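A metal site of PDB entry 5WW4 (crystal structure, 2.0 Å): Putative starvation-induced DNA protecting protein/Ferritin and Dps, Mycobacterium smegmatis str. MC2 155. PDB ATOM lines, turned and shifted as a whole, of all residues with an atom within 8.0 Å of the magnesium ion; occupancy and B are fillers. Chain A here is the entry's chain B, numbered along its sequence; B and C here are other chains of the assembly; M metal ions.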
ATOM      1  N   SER A  47      -2.659  11.921  17.915  1.00  0.00           N
ATOM      2  CA  SER A  47      -3.805  11.352  18.630  1.00  0.00           C
ATOM      3  C   SER A  47      -3.584   9.876  18.968  1.00  0.00           C
ATOM      4  O   SER A  47      -3.339   9.073  18.066  1.00  0.00           O
ATOM      5  CB  SER A  47      -5.054  11.512  17.767  1.00  0.00           C
ATOM      6  OG  SER A  47      -6.147  10.771  18.275  1.00  0.00           O
ATOM      7  N   ASN A  48      -3.672   9.550  20.255  1.00  0.00           N
ATOM      8  CA  ASN A  48      -3.444   8.192  20.773  1.00  0.00           C
ATOM      9  C   ASN A  48      -1.993   7.709  20.605  1.00  0.00           C
ATOM     10  O   ASN A  48      -1.737   6.514  20.402  1.00  0.00           O
ATOM     11  CB  ASN A  48      -4.441   7.183  20.188  1.00  0.00           C
ATOM     12  CG  ASN A  48      -4.619   5.973  21.076  1.00  0.00           C
ATOM     13  OD1 ASN A  48      -4.397   6.047  22.289  1.00  0.00           O
ATOM     14  ND2 ASN A  48      -5.045   4.866  20.496  1.00  0.00           N
ATOM     15  N   PHE A  49      -1.057   8.654  20.702  1.00  0.00           N
ATOM     16  CA  PHE A  49       0.371   8.369  20.664  1.00  0.00           C
ATOM     17  C   PHE A  49       0.758   7.196  21.580  1.00  0.00           C
ATOM     18  O   PHE A  49       1.465   6.283  21.155  1.00  0.00           O
ATOM     19  CB  PHE A  49       1.180   9.609  21.076  1.00  0.00           C
ATOM     20  CG  PHE A  49       2.579   9.292  21.516  1.00  0.00           C
ATOM     21  CD1 PHE A  49       3.577   9.042  20.565  1.00  0.00           C
ATOM     22  CD2 PHE A  49       2.906   9.226  22.880  1.00  0.00           C
ATOM     23  CE1 PHE A  49       4.879   8.741  20.966  1.00  0.00           C
ATOM     24  CE2 PHE A  49       4.205   8.915  23.283  1.00  0.00           C
ATOM     25  CZ  PHE A  49       5.184   8.681  22.329  1.00  0.00           C
ATOM     26  N   ARG A  50       0.300   7.257  22.825  1.00  0.00           N
ATOM     27  CA  ARG A  50       0.815   6.377  23.858  1.00  0.00           C
ATOM     28  C   ARG A  50       0.496   4.911  23.576  1.00  0.00           C
ATOM     29  O   ARG A  50       1.395   4.064  23.659  1.00  0.00           O
ATOM     30  CB  ARG A  50       0.345   6.828  25.242  1.00  0.00           C
ATOM     31  CG  ARG A  50       0.969   6.029  26.378  1.00  0.00           C
ATOM     32  CD  ARG A  50       0.484   6.527  27.720  1.00  0.00           C
ATOM     33  NE  ARG A  50       1.064   5.753  28.821  1.00  0.00           N
ATOM     34  CZ  ARG A  50       0.537   4.636  29.330  1.00  0.00           C
ATOM     35  NH1 ARG A  50      -0.588   4.121  28.834  1.00  0.00           N
ATOM     36  NH2 ARG A  50       1.161   4.025  30.321  1.00  0.00           N
ATOM     37  N   ASP A  51      -0.762   4.613  23.212  1.00  0.00           N
ATOM     38  CA  ASP A  51      -1.177   3.254  22.870  1.00  0.00           C
ATOM     39  C   ASP A  51      -0.356   2.685  21.728  1.00  0.00           C
ATOM     40  O   ASP A  51       0.057   1.505  21.793  1.00  0.00           O
ATOM     41  CB  ASP A  51      -2.658   3.211  22.477  1.00  0.00           C
ATOM     42  CG  ASP A  51      -3.569   2.908  23.654  1.00  0.00           C
ATOM     43  OD1 ASP A  51      -3.204   2.101  24.522  1.00  0.00           O
ATOM     44  OD2 ASP A  51      -4.687   3.471  23.688  1.00  0.00           O
ATOM     45  N   LEU A  52      -0.121   3.494  20.701  1.00  0.00           N
ATOM     46  CA  LEU A  52       0.680   3.058  19.556  1.00  0.00           C
ATOM     47  C   LEU A  52       2.132   2.815  19.925  1.00  0.00           C
ATOM     48  O   LEU A  52       2.661   1.755  19.615  1.00  0.00           O
ATOM     49  CB  LEU A  52       0.572   4.038  18.380  1.00  0.00           C
ATOM     50  CG  LEU A  52      -0.363   3.684  17.201  1.00  0.00           C
ATOM     51  CD1 LEU A  52       0.053   2.365  16.543  1.00  0.00           C
ATOM     52  CD2 LEU A  52      -1.841   3.670  17.607  1.00  0.00           C
ATOM     53  N   LEU A  54       3.342   2.079  22.831  1.00  0.00           N
ATOM     54  CA  LEU A  54       3.348   0.832  23.597  1.00  0.00           C
ATOM     55  C   LEU A  54       3.100  -0.429  22.762  1.00  0.00           C
ATOM     56  O   LEU A  54       3.812  -1.422  22.917  1.00  0.00           O
ATOM     57  CB  LEU A  54       2.361   0.901  24.779  1.00  0.00           C
ATOM     58  CG  LEU A  54       2.674   1.923  25.878  1.00  0.00           C
ATOM     59  CD1 LEU A  54       1.497   2.006  26.865  1.00  0.00           C
ATOM     60  CD2 LEU A  54       3.996   1.636  26.610  1.00  0.00           C
ATOM     61  N   GLU A 157      -7.318   0.558  15.321  1.00  0.00           N
ATOM     62  CA  GLU A 157      -7.288   1.997  15.570  1.00  0.00           C
ATOM     63  C   GLU A 157      -7.914   2.840  14.442  1.00  0.00           C
ATOM     64  O   GLU A 157      -8.586   3.833  14.712  1.00  0.00           O
ATOM     65  CB  GLU A 157      -5.855   2.465  15.866  1.00  0.00           C
ATOM     66  CG  GLU A 157      -5.649   3.986  15.952  1.00  0.00           C
ATOM     67  CD  GLU A 157      -6.223   4.636  17.213  1.00  0.00           C
ATOM     68  OE1 GLU A 157      -6.515   5.853  17.169  1.00  0.00           O
ATOM     69  OE2 GLU A 157      -6.376   3.944  18.240  1.00  0.00           O
ATOM     70  N   SER B  47     -11.217  12.430  24.765  1.00  0.00           N
ATOM     71  CA  SER B  47     -10.531  11.514  23.837  1.00  0.00           C
ATOM     72  C   SER B  47      -9.167  11.085  24.388  1.00  0.00           C
ATOM     73  O   SER B  47      -8.333  11.928  24.736  1.00  0.00           O
ATOM     74  CB  SER B  47     -10.360  12.180  22.470  1.00  0.00           C
ATOM     75  OG  SER B  47      -9.677  11.322  21.560  1.00  0.00           O
ATOM     76  N   ASN B  48      -8.949   9.766  24.460  1.00  0.00           N
ATOM     77  CA  ASN B  48      -7.721   9.189  24.999  1.00  0.00           C
ATOM     78  C   ASN B  48      -7.487   9.438  26.496  1.00  0.00           C
ATOM     79  O   ASN B  48      -6.341   9.544  26.953  1.00  0.00           O
ATOM     80  CB  ASN B  48      -6.479   9.563  24.159  1.00  0.00           C
ATOM     81  CG  ASN B  48      -5.386   8.524  24.280  1.00  0.00           C
ATOM     82  OD1 ASN B  48      -5.667   7.368  24.554  1.00  0.00           O
ATOM     83  ND2 ASN B  48      -4.122   8.940  24.101  1.00  0.00           N
ATOM     84  N   PHE B  49      -8.585   9.514  27.245  1.00  0.00           N
ATOM     85  CA  PHE B  49      -8.546   9.655  28.701  1.00  0.00           C
ATOM     86  C   PHE B  49      -7.601   8.644  29.372  1.00  0.00           C
ATOM     87  O   PHE B  49      -6.765   9.034  30.166  1.00  0.00           O
ATOM     88  CB  PHE B  49      -9.938   9.512  29.325  1.00  0.00           C
ATOM     89  CG  PHE B  49      -9.915   9.157  30.783  1.00  0.00           C
ATOM     90  CD1 PHE B  49      -9.730  10.149  31.749  1.00  0.00           C
ATOM     91  CD2 PHE B  49     -10.032   7.821  31.191  1.00  0.00           C
ATOM     92  CE1 PHE B  49      -9.675   9.824  33.106  1.00  0.00           C
ATOM     93  CE2 PHE B  49      -9.969   7.493  32.543  1.00  0.00           C
ATOM     94  CZ  PHE B  49      -9.802   8.486  33.497  1.00  0.00           C
ATOM     95  N   ARG B  50      -7.746   7.362  29.032  1.00  0.00           N
ATOM     96  CA  ARG B  50      -7.063   6.308  29.761  1.00  0.00           C
ATOM     97  C   ARG B  50      -5.533   6.440  29.669  1.00  0.00           C
ATOM     98  O   ARG B  50      -4.869   6.415  30.704  1.00  0.00           O
ATOM     99  CB  ARG B  50      -7.558   4.926  29.327  1.00  0.00           C
ATOM    100  CG  ARG B  50      -6.998   3.777  30.144  1.00  0.00           C
ATOM    101  CD  ARG B  50      -7.530   2.448  29.668  1.00  0.00           C
ATOM    102  NE  ARG B  50      -6.970   1.348  30.469  1.00  0.00           N
ATOM    103  CZ  ARG B  50      -5.841   0.701  30.197  1.00  0.00           C
ATOM    104  NH1 ARG B  50      -5.108   1.016  29.129  1.00  0.00           N
ATOM    105  NH2 ARG B  50      -5.446  -0.269  30.996  1.00  0.00           N
ATOM    106  N   ASP B  51      -5.002   6.621  28.450  1.00  0.00           N
ATOM    107  CA  ASP B  51      -3.556   6.816  28.262  1.00  0.00           C
ATOM    108  C   ASP B  51      -3.018   7.967  29.097  1.00  0.00           C
ATOM    109  O   ASP B  51      -1.983   7.834  29.754  1.00  0.00           O
ATOM    110  CB  ASP B  51      -3.196   7.080  26.808  1.00  0.00           C
ATOM    111  CG  ASP B  51      -2.880   5.820  26.027  1.00  0.00           C
ATOM    112  OD1 ASP B  51      -2.228   4.907  26.563  1.00  0.00           O
ATOM    113  OD2 ASP B  51      -3.276   5.770  24.852  1.00  0.00           O
ATOM    114  N   LEU B  52      -3.719   9.104  29.059  1.00  0.00           N
ATOM    115  CA  LEU B  52      -3.295  10.295  29.804  1.00  0.00           C
ATOM    116  C   LEU B  52      -3.345  10.065  31.301  1.00  0.00           C
ATOM    117  O   LEU B  52      -2.383  10.374  31.987  1.00  0.00           O
ATOM    118  CB  LEU B  52      -4.110  11.539  29.393  1.00  0.00           C
ATOM    119  CG  LEU B  52      -3.455  12.466  28.351  1.00  0.00           C
ATOM    120  CD1 LEU B  52      -2.081  12.960  28.813  1.00  0.00           C
ATOM    121  CD2 LEU B  52      -3.340  11.812  26.965  1.00  0.00           C
ATOM    122  N   LEU B  54      -3.151   7.191  32.875  1.00  0.00           N
ATOM    123  CA  LEU B  54      -2.025   6.315  33.214  1.00  0.00           C
ATOM    124  C   LEU B  54      -0.655   6.994  33.179  1.00  0.00           C
ATOM    125  O   LEU B  54       0.110   6.879  34.132  1.00  0.00           O
ATOM    126  CB  LEU B  54      -2.032   5.054  32.338  1.00  0.00           C
ATOM    127  CG  LEU B  54      -3.240   4.117  32.494  1.00  0.00           C
ATOM    128  CD1 LEU B  54      -3.202   3.040  31.424  1.00  0.00           C
ATOM    129  CD2 LEU B  54      -3.331   3.490  33.893  1.00  0.00           C
ATOM    130  N   GLU B 157       0.915  13.396  22.097  1.00  0.00           N
ATOM    131  CA  GLU B 157      -0.534  13.290  21.911  1.00  0.00           C
ATOM    132  C   GLU B 157      -1.123  14.434  21.087  1.00  0.00           C
ATOM    133  O   GLU B 157      -1.991  14.200  20.249  1.00  0.00           O
ATOM    134  CB  GLU B 157      -1.248  13.205  23.279  1.00  0.00           C
ATOM    135  CG  GLU B 157      -2.781  13.306  23.279  1.00  0.00           C
ATOM    136  CD  GLU B 157      -3.481  12.137  22.581  1.00  0.00           C
ATOM    137  OE1 GLU B 157      -4.608  12.363  22.069  1.00  0.00           O
ATOM    138  OE2 GLU B 157      -2.947  11.014  22.538  1.00  0.00           O
ATOM    139  N   SER C  47     -11.018   4.750  16.928  1.00  0.00           N
ATOM    140  CA  SER C  47     -10.158   5.669  17.689  1.00  0.00           C
ATOM    141  C   SER C  47     -10.018   5.264  19.156  1.00  0.00           C
ATOM    142  O   SER C  47     -11.007   5.107  19.857  1.00  0.00           O
ATOM    143  CB  SER C  47     -10.687   7.102  17.571  1.00  0.00           C
ATOM    144  OG  SER C  47      -9.851   8.033  18.229  1.00  0.00           O
ATOM    145  N   ASN C  48      -8.762   5.106  19.613  1.00  0.00           N
ATOM    146  CA  ASN C  48      -8.429   4.643  20.968  1.00  0.00           C
ATOM    147  C   ASN C  48      -8.860   3.202  21.262  1.00  0.00           C
ATOM    148  O   ASN C  48      -9.240   2.875  22.401  1.00  0.00           O
ATOM    149  CB  ASN C  48      -8.935   5.599  22.079  1.00  0.00           C
ATOM    150  CG  ASN C  48      -8.052   5.566  23.315  1.00  0.00           C
ATOM    151  OD1 ASN C  48      -6.872   5.197  23.229  1.00  0.00           O
ATOM    152  ND2 ASN C  48      -8.605   5.928  24.468  1.00  0.00           N
ATOM    153  N   PHE C  49      -8.805   2.364  20.228  1.00  0.00           N
ATOM    154  CA  PHE C  49      -9.095   0.929  20.351  1.00  0.00           C
ATOM    155  C   PHE C  49      -8.384   0.303  21.548  1.00  0.00           C
ATOM    156  O   PHE C  49      -9.024  -0.295  22.388  1.00  0.00           O
ATOM    157  CB  PHE C  49      -8.694   0.171  19.071  1.00  0.00           C
ATOM    158  CG  PHE C  49      -8.587  -1.321  19.268  1.00  0.00           C
ATOM    159  CD1 PHE C  49      -7.331  -1.937  19.382  1.00  0.00           C
ATOM    160  CD2 PHE C  49      -9.731  -2.123  19.352  1.00  0.00           C
ATOM    161  CE1 PHE C  49      -7.225  -3.311  19.579  1.00  0.00           C
ATOM    162  CE2 PHE C  49      -9.630  -3.498  19.540  1.00  0.00           C
ATOM    163  CZ  PHE C  49      -8.369  -4.095  19.649  1.00  0.00           C
ATOM    164  N   ARG C  50      -7.055   0.461  21.600  1.00  0.00           N
ATOM    165  CA  ARG C  50      -6.226  -0.282  22.537  1.00  0.00           C
ATOM    166  C   ARG C  50      -6.614  -0.025  23.999  1.00  0.00           C
ATOM    167  O   ARG C  50      -6.781  -0.969  24.773  1.00  0.00           O
ATOM    168  CB  ARG C  50      -4.731  -0.009  22.290  1.00  0.00           C
ATOM    169  CG  ARG C  50      -3.801  -0.915  23.107  1.00  0.00           C
ATOM    170  CD  ARG C  50      -2.346  -0.723  22.707  1.00  0.00           C
ATOM    171  NE  ARG C  50      -1.455  -1.518  23.546  1.00  0.00           N
ATOM    172  CZ  ARG C  50      -1.004  -1.156  24.751  1.00  0.00           C
ATOM    173  NH1 ARG C  50      -1.379   0.001  25.311  1.00  0.00           N
ATOM    174  NH2 ARG C  50      -0.189  -1.974  25.417  1.00  0.00           N
ATOM    175  N   ASP C  51      -6.772   1.246  24.358  1.00  0.00           N
ATOM    176  CA  ASP C  51      -7.177   1.630  25.713  1.00  0.00           C
ATOM    177  C   ASP C  51      -8.489   0.984  26.115  1.00  0.00           C
ATOM    178  O   ASP C  51      -8.601   0.462  27.228  1.00  0.00           O
ATOM    179  CB  ASP C  51      -7.306   3.146  25.847  1.00  0.00           C
ATOM    180  CG  ASP C  51      -6.048   3.813  26.368  1.00  0.00           C
ATOM    181  OD1 ASP C  51      -5.278   3.194  27.141  1.00  0.00           O
ATOM    182  OD2 ASP C  51      -5.829   4.980  25.989  1.00  0.00           O
ATOM    183  N   LEU C  52      -9.477   1.012  25.212  1.00  0.00           N
ATOM    184  CA  LEU C  52     -10.781   0.410  25.456  1.00  0.00           C
ATOM    185  C   LEU C  52     -10.732  -1.106  25.538  1.00  0.00           C
ATOM    186  O   LEU C  52     -11.281  -1.693  26.476  1.00  0.00           O
ATOM    187  CB  LEU C  52     -11.816   0.848  24.401  1.00  0.00           C
ATOM    188  CG  LEU C  52     -12.750   2.006  24.753  1.00  0.00           C
ATOM    189  CD1 LEU C  52     -13.537   1.683  26.024  1.00  0.00           C
ATOM    190  CD2 LEU C  52     -11.991   3.332  24.863  1.00  0.00           C
ATOM    191  N   GLU C 157     -13.745   8.737  28.332  1.00  0.00           N
ATOM    192  CA  GLU C 157     -13.387   8.784  26.901  1.00  0.00           C
ATOM    193  C   GLU C 157     -14.339   9.660  26.065  1.00  0.00           C
ATOM    194  O   GLU C 157     -13.878  10.402  25.183  1.00  0.00           O
ATOM    195  CB  GLU C 157     -13.351   7.345  26.340  1.00  0.00           C
ATOM    196  CG  GLU C 157     -13.112   7.224  24.832  1.00  0.00           C
ATOM    197  CD  GLU C 157     -11.756   7.752  24.349  1.00  0.00           C
ATOM    198  OE1 GLU C 157     -10.741   7.685  25.080  1.00  0.00           O
ATOM    199  OE2 GLU C 157     -11.706   8.251  23.203  1.00  0.00           O
HETATM  200 MG    MG M   1      -5.100   5.456  24.115  1.00  0.00          MG
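NH1 of Arg 50 of chain A lies within salt-bridge range of OD1 of Asp 51 of chain B. ND2 of Asn 48 of chain C lies within hydrogen-bond range of OE1 of Glu 157 of chain C (2.8 Å). OE2 of Glu 157 of chain A sits at hydrogen-bond distance from N of Asn 48 of chain C, at 3.0 Å. OE1 of Glu 157 of chain C is in hydrogen-bond range of N of Asn 48 of chain B (2.8 Å). The side-chain amide nitrogen (ND2) of Asn 48 of chain B sits at hydrogen-bond distance from the side-chain carboxylate (OE2) of Glu 157 of chain B. The side-chain carboxylate (OE2) of Glu 157 of chain B sits at hydrogen-bond distance from the backbone NH (N) of Asn 48 of chain A (2.8 Å). OE2 of Glu 157 of chain A is in hydrogen-bond range of ND2 of Asn 48 of chain A, at 2.8 Å. The side-chain carboxylate (OD1) of Asp 51 of chain A is in salt-bridge range of the guanidinium group (NH1) of Arg 50 of chain C, 2.9 Å away.
Of the 23 residues printed, 6 come within 4 Å of the magnesium ion. The nearest printed residue that does not touch the magnesium ion is Arg 50 of chain A (5.6 Å).
The magnesium ion is bound by the side-chain carboxylate (OD2) of Asp 51 of chain B (2.0 Å). The side-chain amide oxygen (OD1) of Asn 48 of chain C is bound to the magnesium ion (2.0 Å). OD1 of Asn 48 of chain B binds the magnesium ion (2.0 Å). The magnesium ion is bound by OD1 of Asn 48 of chain A, at 2.0 Å. The side-chain carboxylate (OD2) of Asp 51 of chain C binds the magnesium ion, 2.1 Å away. The magnesium ion is bound by the side-chain carboxylate (OD2) of Asp 51 of chain A, 2.1 Å away.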
